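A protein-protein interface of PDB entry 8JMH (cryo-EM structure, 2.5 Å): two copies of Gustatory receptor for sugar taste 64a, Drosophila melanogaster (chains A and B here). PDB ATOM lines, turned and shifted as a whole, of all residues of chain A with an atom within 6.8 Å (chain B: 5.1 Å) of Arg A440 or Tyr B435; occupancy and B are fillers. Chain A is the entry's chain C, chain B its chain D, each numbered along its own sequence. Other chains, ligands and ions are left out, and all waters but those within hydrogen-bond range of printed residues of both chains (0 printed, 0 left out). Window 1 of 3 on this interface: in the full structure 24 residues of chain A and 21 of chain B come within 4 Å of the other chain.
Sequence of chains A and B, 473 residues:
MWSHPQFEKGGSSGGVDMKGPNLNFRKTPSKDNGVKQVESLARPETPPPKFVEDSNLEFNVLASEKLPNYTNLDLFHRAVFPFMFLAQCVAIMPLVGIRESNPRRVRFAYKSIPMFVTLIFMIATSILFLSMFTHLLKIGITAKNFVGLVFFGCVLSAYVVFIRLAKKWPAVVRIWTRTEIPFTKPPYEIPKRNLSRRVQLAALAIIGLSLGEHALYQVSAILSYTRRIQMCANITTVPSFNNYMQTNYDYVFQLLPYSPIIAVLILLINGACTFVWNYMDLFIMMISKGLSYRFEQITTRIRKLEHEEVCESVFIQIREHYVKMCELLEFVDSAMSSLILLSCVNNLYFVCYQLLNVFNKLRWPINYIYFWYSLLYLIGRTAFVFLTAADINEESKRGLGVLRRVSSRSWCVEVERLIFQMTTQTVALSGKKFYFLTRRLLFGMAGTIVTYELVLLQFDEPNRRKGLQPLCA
Of the 12 printed residues of chain A, 4 touch a printed residue of chain B.
Printed residues of chain A that touch a printed residue of chain B: Arg A439, Arg A440, Leu A442 and Phe A443.
Hydrophobic or aromatic side chains of chain A that line the printed part of chain B: Leu A442 and Phe A443.
Of the 12 printed residues of chain B, 3 touch a printed residue of chain A.
Hydrophobic or aromatic side chains of chain B within 4 Å of the printed part of chain A: Phe B434 and Tyr B435.
Among the printed residues, 7 pairs touch across the chains.
O of Phe B434 lies within hydrogen-bond range of NH1 of Arg A440 (2.5 Å).
3 positions are printed for both chains.
Of the 7 pairs that touch across the chains among the printed residues, none has its exchanged pair printed and touching as well.
Of chain B, only Phe B434 and Tyr B435 come within 4 Å of Arg A440.
Of chain A, only Arg A440 (3.7 Å) and Phe A443 (3.7 Å) come within 4 Å of Tyr B435.
Printed residues of chain B within 4 Å of Arg A439: Lys B433 and Phe B434.
Of the printed residues of chain A, Phe B434 touches Arg A439, Arg A440, Leu A442 and Phe A443.
Printed residues of chain B within 4 Å of Phe A443: Phe B434 and Tyr B435.
Printed residues of chain A within 4 Å of Lys B433: Arg A439.
Leu A437 touches none of the printed residues of chain B.
The nearest residue of chain A that does not touch Tyr B435 is Arg A439 (5.8 Å).
The side-chain sulfur (SG) of Cys B344 is in hydrogen-bond range of the side-chain hydroxyl (OH) of Tyr B435 (3.0 Å).
OG of Ser B430 sits at hydrogen-bond distance from N of Lys B433 (3.1 Å).
O of Lys B433 touches CB of Arg A439, 3.7 Å away.
CD1 of Phe B434 touches O of Arg A439, 3.3 Å away.
CA of Tyr B435 touches NH1 of Arg A440 (3.7 Å).
Leu A442 touches Phe B434 (CD2 to CE1, 3.8 Å).
Phe A443 touches Phe B434 (CB to O, 3.5 Å).
Phe A443 touches Tyr B435.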
ATOM      1  N   ALA A 390     -21.903 -14.761  28.240  1.00  0.00           N
ATOM      2  CA  ALA A 390     -23.123 -14.347  27.561  1.00  0.00           C
ATOM      3  C   ALA A 390     -24.328 -15.181  27.967  1.00  0.00           C
ATOM      4  O   ALA A 390     -25.463 -14.737  27.769  1.00  0.00           O
ATOM      5  CB  ALA A 390     -22.933 -14.428  26.047  1.00  0.00           C
ATOM      6  N   GLU A 394     -28.354 -14.406  28.144  1.00  0.00           N
ATOM      7  CA  GLU A 394     -29.336 -15.234  27.453  1.00  0.00           C
ATOM      8  C   GLU A 394     -30.332 -15.842  28.430  1.00  0.00           C
ATOM      9  O   GLU A 394     -31.535 -15.895  28.150  1.00  0.00           O
ATOM     10  CB  GLU A 394     -28.629 -16.334  26.660  1.00  0.00           C
ATOM     11  CG  GLU A 394     -27.746 -15.819  25.537  1.00  0.00           C
ATOM     12  CD  GLU A 394     -28.513 -15.000  24.518  1.00  0.00           C
ATOM     13  OE1 GLU A 394     -29.682 -15.338  24.242  1.00  0.00           O
ATOM     14  OE2 GLU A 394     -27.947 -14.017  23.997  1.00  0.00           O
ATOM     15  N   PHE A 436     -20.459  -5.140  27.246  1.00  0.00           N
ATOM     16  CA  PHE A 436     -21.165  -6.172  27.991  1.00  0.00           C
ATOM     17  C   PHE A 436     -20.967  -7.508  27.294  1.00  0.00           C
ATOM     18  O   PHE A 436     -21.117  -7.604  26.072  1.00  0.00           O
ATOM     19  CB  PHE A 436     -22.652  -5.839  28.111  1.00  0.00           C
ATOM     20  CG  PHE A 436     -22.936  -4.694  29.037  1.00  0.00           C
ATOM     21  CD1 PHE A 436     -22.810  -3.389  28.599  1.00  0.00           C
ATOM     22  CD2 PHE A 436     -23.317  -4.922  30.347  1.00  0.00           C
ATOM     23  CE1 PHE A 436     -23.063  -2.332  29.447  1.00  0.00           C
ATOM     24  CE2 PHE A 436     -23.573  -3.870  31.200  1.00  0.00           C
ATOM     25  CZ  PHE A 436     -23.446  -2.572  30.750  1.00  0.00           C
ATOM     26  N   LEU A 437     -20.631  -8.533  28.071  1.00  0.00           N
ATOM     27  CA  LEU A 437     -20.366  -9.858  27.519  1.00  0.00           C
ATOM     28  C   LEU A 437     -21.687 -10.473  27.082  1.00  0.00           C
ATOM     29  O   LEU A 437     -22.392 -11.098  27.876  1.00  0.00           O
ATOM     30  CB  LEU A 437     -19.658 -10.733  28.548  1.00  0.00           C
ATOM     31  CG  LEU A 437     -18.290 -10.237  29.022  1.00  0.00           C
ATOM     32  CD1 LEU A 437     -17.670 -11.228  29.991  1.00  0.00           C
ATOM     33  CD2 LEU A 437     -17.361  -9.997  27.848  1.00  0.00           C
ATOM     34  N   THR A 438     -22.024 -10.289  25.810  1.00  0.00           N
ATOM     35  CA  THR A 438     -23.227 -10.839  25.205  1.00  0.00           C
ATOM     36  C   THR A 438     -22.834 -11.558  23.920  1.00  0.00           C
ATOM     37  O   THR A 438     -21.679 -11.519  23.491  1.00  0.00           O
ATOM     38  CB  THR A 438     -24.259  -9.740  24.922  1.00  0.00           C
ATOM     39  OG1 THR A 438     -23.689  -8.758  24.048  1.00  0.00           O
ATOM     40  CG2 THR A 438     -24.695  -9.067  26.213  1.00  0.00           C
ATOM     41  N   ARG A 439     -23.807 -12.226  23.302  1.00  0.00           N
ATOM     42  CA  ARG A 439     -23.537 -12.890  22.032  1.00  0.00           C
ATOM     43  C   ARG A 439     -23.306 -11.879  20.918  1.00  0.00           C
ATOM     44  O   ARG A 439     -22.554 -12.151  19.977  1.00  0.00           O
ATOM     45  CB  ARG A 439     -24.685 -13.831  21.675  1.00  0.00           C
ATOM     46  CG  ARG A 439     -24.792 -15.032  22.596  1.00  0.00           C
ATOM     47  CD  ARG A 439     -25.448 -16.215  21.912  1.00  0.00           C
ATOM     48  NE  ARG A 439     -25.085 -17.473  22.552  1.00  0.00           N
ATOM     49  CZ  ARG A 439     -24.956 -18.633  21.923  1.00  0.00           C
ATOM     50  NH1 ARG A 439     -25.160 -18.743  20.620  1.00  0.00           N
ATOM     51  NH2 ARG A 439     -24.611 -19.712  22.617  1.00  0.00           N
ATOM     52  N   ARG A 440     -23.943 -10.710  21.004  1.00  0.00           N
ATOM     53  CA  ARG A 440     -23.684  -9.661  20.026  1.00  0.00           C
ATOM     54  C   ARG A 440     -22.237  -9.193  20.098  1.00  0.00           C
ATOM     55  O   ARG A 440     -21.607  -8.935  19.066  1.00  0.00           O
ATOM     56  CB  ARG A 440     -24.636  -8.485  20.248  1.00  0.00           C
ATOM     57  CG  ARG A 440     -26.111  -8.843  20.146  1.00  0.00           C
ATOM     58  CD  ARG A 440     -26.531  -9.123  18.712  1.00  0.00           C
ATOM     59  NE  ARG A 440     -26.392  -7.949  17.855  1.00  0.00           N
ATOM     60  CZ  ARG A 440     -25.616  -7.873  16.779  1.00  0.00           C
ATOM     61  NH1 ARG A 440     -24.874  -8.894  16.381  1.00  0.00           N
ATOM     62  NH2 ARG A 440     -25.584  -6.740  16.083  1.00  0.00           N
ATOM     63  N   LEU A 441     -21.693  -9.073  21.310  1.00  0.00           N
ATOM     64  CA  LEU A 441     -20.309  -8.636  21.457  1.00  0.00           C
ATOM     65  C   LEU A 441     -19.342  -9.641  20.843  1.00  0.00           C
ATOM     66  O   LEU A 441     -18.372  -9.250  20.185  1.00  0.00           O
ATOM     67  CB  LEU A 441     -19.982  -8.415  22.933  1.00  0.00           C
ATOM     68  CG  LEU A 441     -18.582  -7.871  23.229  1.00  0.00           C
ATOM     69  CD1 LEU A 441     -18.524  -6.377  22.967  1.00  0.00           C
ATOM     70  CD2 LEU A 441     -18.179  -8.184  24.658  1.00  0.00           C
ATOM     71  N   LEU A 442     -19.585 -10.935  21.047  1.00  0.00           N
ATOM     72  CA  LEU A 442     -18.712 -11.943  20.457  1.00  0.00           C
ATOM     73  C   LEU A 442     -18.750 -11.871  18.939  1.00  0.00           C
ATOM     74  O   LEU A 442     -17.720 -12.038  18.274  1.00  0.00           O
ATOM     75  CB  LEU A 442     -19.110 -13.336  20.942  1.00  0.00           C
ATOM     76  CG  LEU A 442     -18.198 -14.486  20.502  1.00  0.00           C
ATOM     77  CD1 LEU A 442     -16.760 -14.246  20.935  1.00  0.00           C
ATOM     78  CD2 LEU A 442     -18.707 -15.806  21.052  1.00  0.00           C
ATOM     79  N   PHE A 443     -19.931 -11.627  18.368  1.00  0.00           N
ATOM     80  CA  PHE A 443     -20.015 -11.379  16.935  1.00  0.00           C
ATOM     81  C   PHE A 443     -19.238 -10.125  16.554  1.00  0.00           C
ATOM     82  O   PHE A 443     -18.528 -10.109  15.543  1.00  0.00           O
ATOM     83  CB  PHE A 443     -21.479 -11.249  16.514  1.00  0.00           C
ATOM     84  CG  PHE A 443     -21.680 -11.198  15.028  1.00  0.00           C
ATOM     85  CD1 PHE A 443     -21.227 -12.224  14.217  1.00  0.00           C
ATOM     86  CD2 PHE A 443     -22.323 -10.122  14.442  1.00  0.00           C
ATOM     87  CE1 PHE A 443     -21.411 -12.176  12.852  1.00  0.00           C
ATOM     88  CE2 PHE A 443     -22.510 -10.071  13.077  1.00  0.00           C
ATOM     89  CZ  PHE A 443     -22.054 -11.099  12.281  1.00  0.00           C
ATOM     90  N   GLY A 444     -19.361  -9.065  17.352  1.00  0.00           N
ATOM     91  CA  GLY A 444     -18.587  -7.864  17.092  1.00  0.00           C
ATOM     92  C   GLY A 444     -17.096  -8.092  17.245  1.00  0.00           C
ATOM     93  O   GLY A 444     -16.294  -7.543  16.486  1.00  0.00           O
ATOM     94  N   MET A 445     -16.704  -8.901  18.231  1.00  0.00           N
ATOM     95  CA  MET A 445     -15.291  -9.227  18.397  1.00  0.00           C
ATOM     96  C   MET A 445     -14.755  -9.973  17.185  1.00  0.00           C
ATOM     97  O   MET A 445     -13.656  -9.678  16.701  1.00  0.00           O
ATOM     98  CB  MET A 445     -15.093 -10.058  19.664  1.00  0.00           C
ATOM     99  CG  MET A 445     -13.735  -9.875  20.317  1.00  0.00           C
ATOM    100  SD  MET A 445     -13.139 -11.381  21.106  1.00  0.00           S
ATOM    101  CE  MET A 445     -11.702 -10.761  21.976  1.00  0.00           C
ATOM    102  N   ILE B 340     -28.722 -21.120   9.355  1.00  0.00           N
ATOM    103  CA  ILE B 340     -28.631 -19.690   9.079  1.00  0.00           C
ATOM    104  C   ILE B 340     -27.182 -19.229   9.173  1.00  0.00           C
ATOM    105  O   ILE B 340     -26.694 -18.478   8.321  1.00  0.00           O
ATOM    106  CB  ILE B 340     -29.536 -18.897  10.038  1.00  0.00           C
ATOM    107  CG1 ILE B 340     -31.008 -19.166   9.722  1.00  0.00           C
ATOM    108  CG2 ILE B 340     -29.238 -17.409   9.940  1.00  0.00           C
ATOM    109  CD1 ILE B 340     -31.945 -18.819  10.855  1.00  0.00           C
ATOM    110  N   LEU B 341     -26.474 -19.673  10.211  1.00  0.00           N
ATOM    111  CA  LEU B 341     -25.086 -19.266  10.395  1.00  0.00           C
ATOM    112  C   LEU B 341     -24.217 -19.749   9.238  1.00  0.00           C
ATOM    113  O   LEU B 341     -23.409 -18.988   8.689  1.00  0.00           O
ATOM    114  CB  LEU B 341     -24.572 -19.808  11.728  1.00  0.00           C
ATOM    115  CG  LEU B 341     -23.380 -19.110  12.379  1.00  0.00           C
ATOM    116  CD1 LEU B 341     -23.728 -17.680  12.756  1.00  0.00           C
ATOM    117  CD2 LEU B 341     -22.926 -19.889  13.600  1.00  0.00           C
ATOM    118  N   CYS B 344     -25.045 -17.792   6.053  1.00  0.00           N
ATOM    119  CA  CYS B 344     -24.541 -16.425   6.104  1.00  0.00           C
ATOM    120  C   CYS B 344     -23.036 -16.387   5.880  1.00  0.00           C
ATOM    121  O   CYS B 344     -22.537 -15.576   5.092  1.00  0.00           O
ATOM    122  CB  CYS B 344     -24.901 -15.787   7.445  1.00  0.00           C
ATOM    123  SG  CYS B 344     -26.670 -15.506   7.678  1.00  0.00           S
ATOM    124  N   LEU B 429     -35.462 -14.091  12.861  1.00  0.00           N
ATOM    125  CA  LEU B 429     -34.529 -15.204  12.869  1.00  0.00           C
ATOM    126  C   LEU B 429     -33.127 -14.706  13.206  1.00  0.00           C
ATOM    127  O   LEU B 429     -32.767 -13.556  12.944  1.00  0.00           O
ATOM    128  CB  LEU B 429     -34.527 -15.910  11.513  1.00  0.00           C
ATOM    129  CG  LEU B 429     -35.821 -16.626  11.121  1.00  0.00           C
ATOM    130  CD1 LEU B 429     -35.768 -17.062   9.668  1.00  0.00           C
ATOM    131  CD2 LEU B 429     -36.074 -17.821  12.025  1.00  0.00           C
ATOM    132  N   SER B 430     -32.328 -15.590  13.801  1.00  0.00           N
ATOM    133  CA  SER B 430     -31.008 -15.208  14.276  1.00  0.00           C
ATOM    134  C   SER B 430     -30.015 -16.326  14.003  1.00  0.00           C
ATOM    135  O   SER B 430     -30.372 -17.506  13.984  1.00  0.00           O
ATOM    136  CB  SER B 430     -31.030 -14.883  15.773  1.00  0.00           C
ATOM    137  OG  SER B 430     -31.132 -16.065  16.546  1.00  0.00           O
ATOM    138  N   GLY B 431     -28.763 -15.934  13.785  1.00  0.00           N
ATOM    139  CA  GLY B 431     -27.666 -16.873  13.662  1.00  0.00           C
ATOM    140  C   GLY B 431     -27.089 -17.252  15.010  1.00  0.00           C
ATOM    141  O   GLY B 431     -26.036 -16.742  15.399  1.00  0.00           O
ATOM    142  N   LYS B 433     -28.271 -16.346  17.758  1.00  0.00           N
ATOM    143  CA  LYS B 433     -28.427 -15.119  18.532  1.00  0.00           C
ATOM    144  C   LYS B 433     -27.224 -14.193  18.418  1.00  0.00           C
ATOM    145  O   LYS B 433     -27.201 -13.140  19.066  1.00  0.00           O
ATOM    146  CB  LYS B 433     -28.700 -15.411  20.011  1.00  0.00           C
ATOM    147  CG  LYS B 433     -29.886 -16.329  20.259  1.00  0.00           C
ATOM    148  CD  LYS B 433     -31.173 -15.533  20.397  1.00  0.00           C
ATOM    149  CE  LYS B 433     -32.401 -16.421  20.278  1.00  0.00           C
ATOM    150  NZ  LYS B 433     -33.538 -15.708  19.634  1.00  0.00           N
ATOM    151  N   PHE B 434     -26.219 -14.550  17.615  1.00  0.00           N
ATOM    152  CA  PHE B 434     -25.105 -13.640  17.383  1.00  0.00           C
ATOM    153  C   PHE B 434     -25.547 -12.421  16.590  1.00  0.00           C
ATOM    154  O   PHE B 434     -24.995 -11.330  16.767  1.00  0.00           O
ATOM    155  CB  PHE B 434     -23.980 -14.367  16.648  1.00  0.00           C
ATOM    156  CG  PHE B 434     -23.337 -15.455  17.451  1.00  0.00           C
ATOM    157  CD1 PHE B 434     -22.694 -15.169  18.641  1.00  0.00           C
ATOM    158  CD2 PHE B 434     -23.375 -16.766  17.016  1.00  0.00           C
ATOM    159  CE1 PHE B 434     -22.102 -16.170  19.380  1.00  0.00           C
ATOM    160  CE2 PHE B 434     -22.785 -17.771  17.751  1.00  0.00           C
ATOM    161  CZ  PHE B 434     -22.148 -17.473  18.934  1.00  0.00           C
ATOM    162  N   TYR B 435     -26.530 -12.591  15.712  1.00  0.00           N
ATOM    163  CA  TYR B 435     -27.101 -11.493  14.951  1.00  0.00           C
ATOM    164  C   TYR B 435     -28.524 -11.877  14.585  1.00  0.00           C
ATOM    165  O   TYR B 435     -28.880 -13.057  14.570  1.00  0.00           O
ATOM    166  CB  TYR B 435     -26.279 -11.189  13.695  1.00  0.00           C
ATOM    167  CG  TYR B 435     -26.054 -12.397  12.816  1.00  0.00           C
ATOM    168  CD1 TYR B 435     -24.951 -13.216  13.000  1.00  0.00           C
ATOM    169  CD2 TYR B 435     -26.947 -12.720  11.807  1.00  0.00           C
ATOM    170  CE1 TYR B 435     -24.742 -14.321  12.202  1.00  0.00           C
ATOM    171  CE2 TYR B 435     -26.747 -13.822  11.005  1.00  0.00           C
ATOM    172  CZ  TYR B 435     -25.644 -14.619  11.206  1.00  0.00           C
ATOM    173  OH  TYR B 435     -25.441 -15.719  10.408  1.00  0.00           O
ATOM    174  N   PHE B 436     -29.335 -10.867  14.287  1.00  0.00           N
ATOM    175  CA  PHE B 436     -30.735 -11.061  13.939  1.00  0.00           C
ATOM    176  C   PHE B 436     -30.959 -10.606  12.508  1.00  0.00           C
ATOM    177  O   PHE B 436     -30.520  -9.517  12.123  1.00  0.00           O
ATOM    178  CB  PHE B 436     -31.647 -10.297  14.899  1.00  0.00           C
ATOM    179  CG  PHE B 436     -31.698 -10.890  16.275  1.00  0.00           C
ATOM    180  CD1 PHE B 436     -30.707 -10.612  17.198  1.00  0.00           C
ATOM    181  CD2 PHE B 436     -32.730 -11.737  16.642  1.00  0.00           C
ATOM    182  CE1 PHE B 436     -30.747 -11.160  18.463  1.00  0.00           C
ATOM    183  CE2 PHE B 436     -32.774 -12.287  17.905  1.00  0.00           C
ATOM    184  CZ  PHE B 436     -31.782 -11.998  18.817  1.00  0.00           C
ATOM    185  N   LEU B 437     -31.641 -11.435  11.725  1.00  0.00           N
ATOM    186  CA  LEU B 437     -31.866 -11.149  10.312  1.00  0.00           C
ATOM    187  C   LEU B 437     -32.878 -10.019  10.197  1.00  0.00           C
ATOM    188  O   LEU B 437     -34.090 -10.242  10.215  1.00  0.00           O
ATOM    189  CB  LEU B 437     -32.344 -12.400   9.584  1.00  0.00           C
ATOM    190  CG  LEU B 437     -31.371 -13.583   9.585  1.00  0.00           C
ATOM    191  CD1 LEU B 437     -31.930 -14.744   8.785  1.00  0.00           C
ATOM    192  CD2 LEU B 437     -30.018 -13.170   9.035  1.00  0.00           C
ATOM    193  N   LEU B 441     -29.390  -5.361   9.670  1.00  0.00           N
ATOM    194  CA  LEU B 441     -28.318  -6.336   9.508  1.00  0.00           C
ATOM    195  C   LEU B 441     -27.866  -6.423   8.057  1.00  0.00           C
ATOM    196  O   LEU B 441     -26.676  -6.591   7.787  1.00  0.00           O
ATOM    197  CB  LEU B 441     -28.762  -7.709  10.009  1.00  0.00           C
ATOM    198  CG  LEU B 441     -27.666  -8.778   9.964  1.00  0.00           C
ATOM    199  CD1 LEU B 441     -26.699  -8.591  11.119  1.00  0.00           C
ATOM    200  CD2 LEU B 441     -28.259 -10.173   9.982  1.00  0.00           C
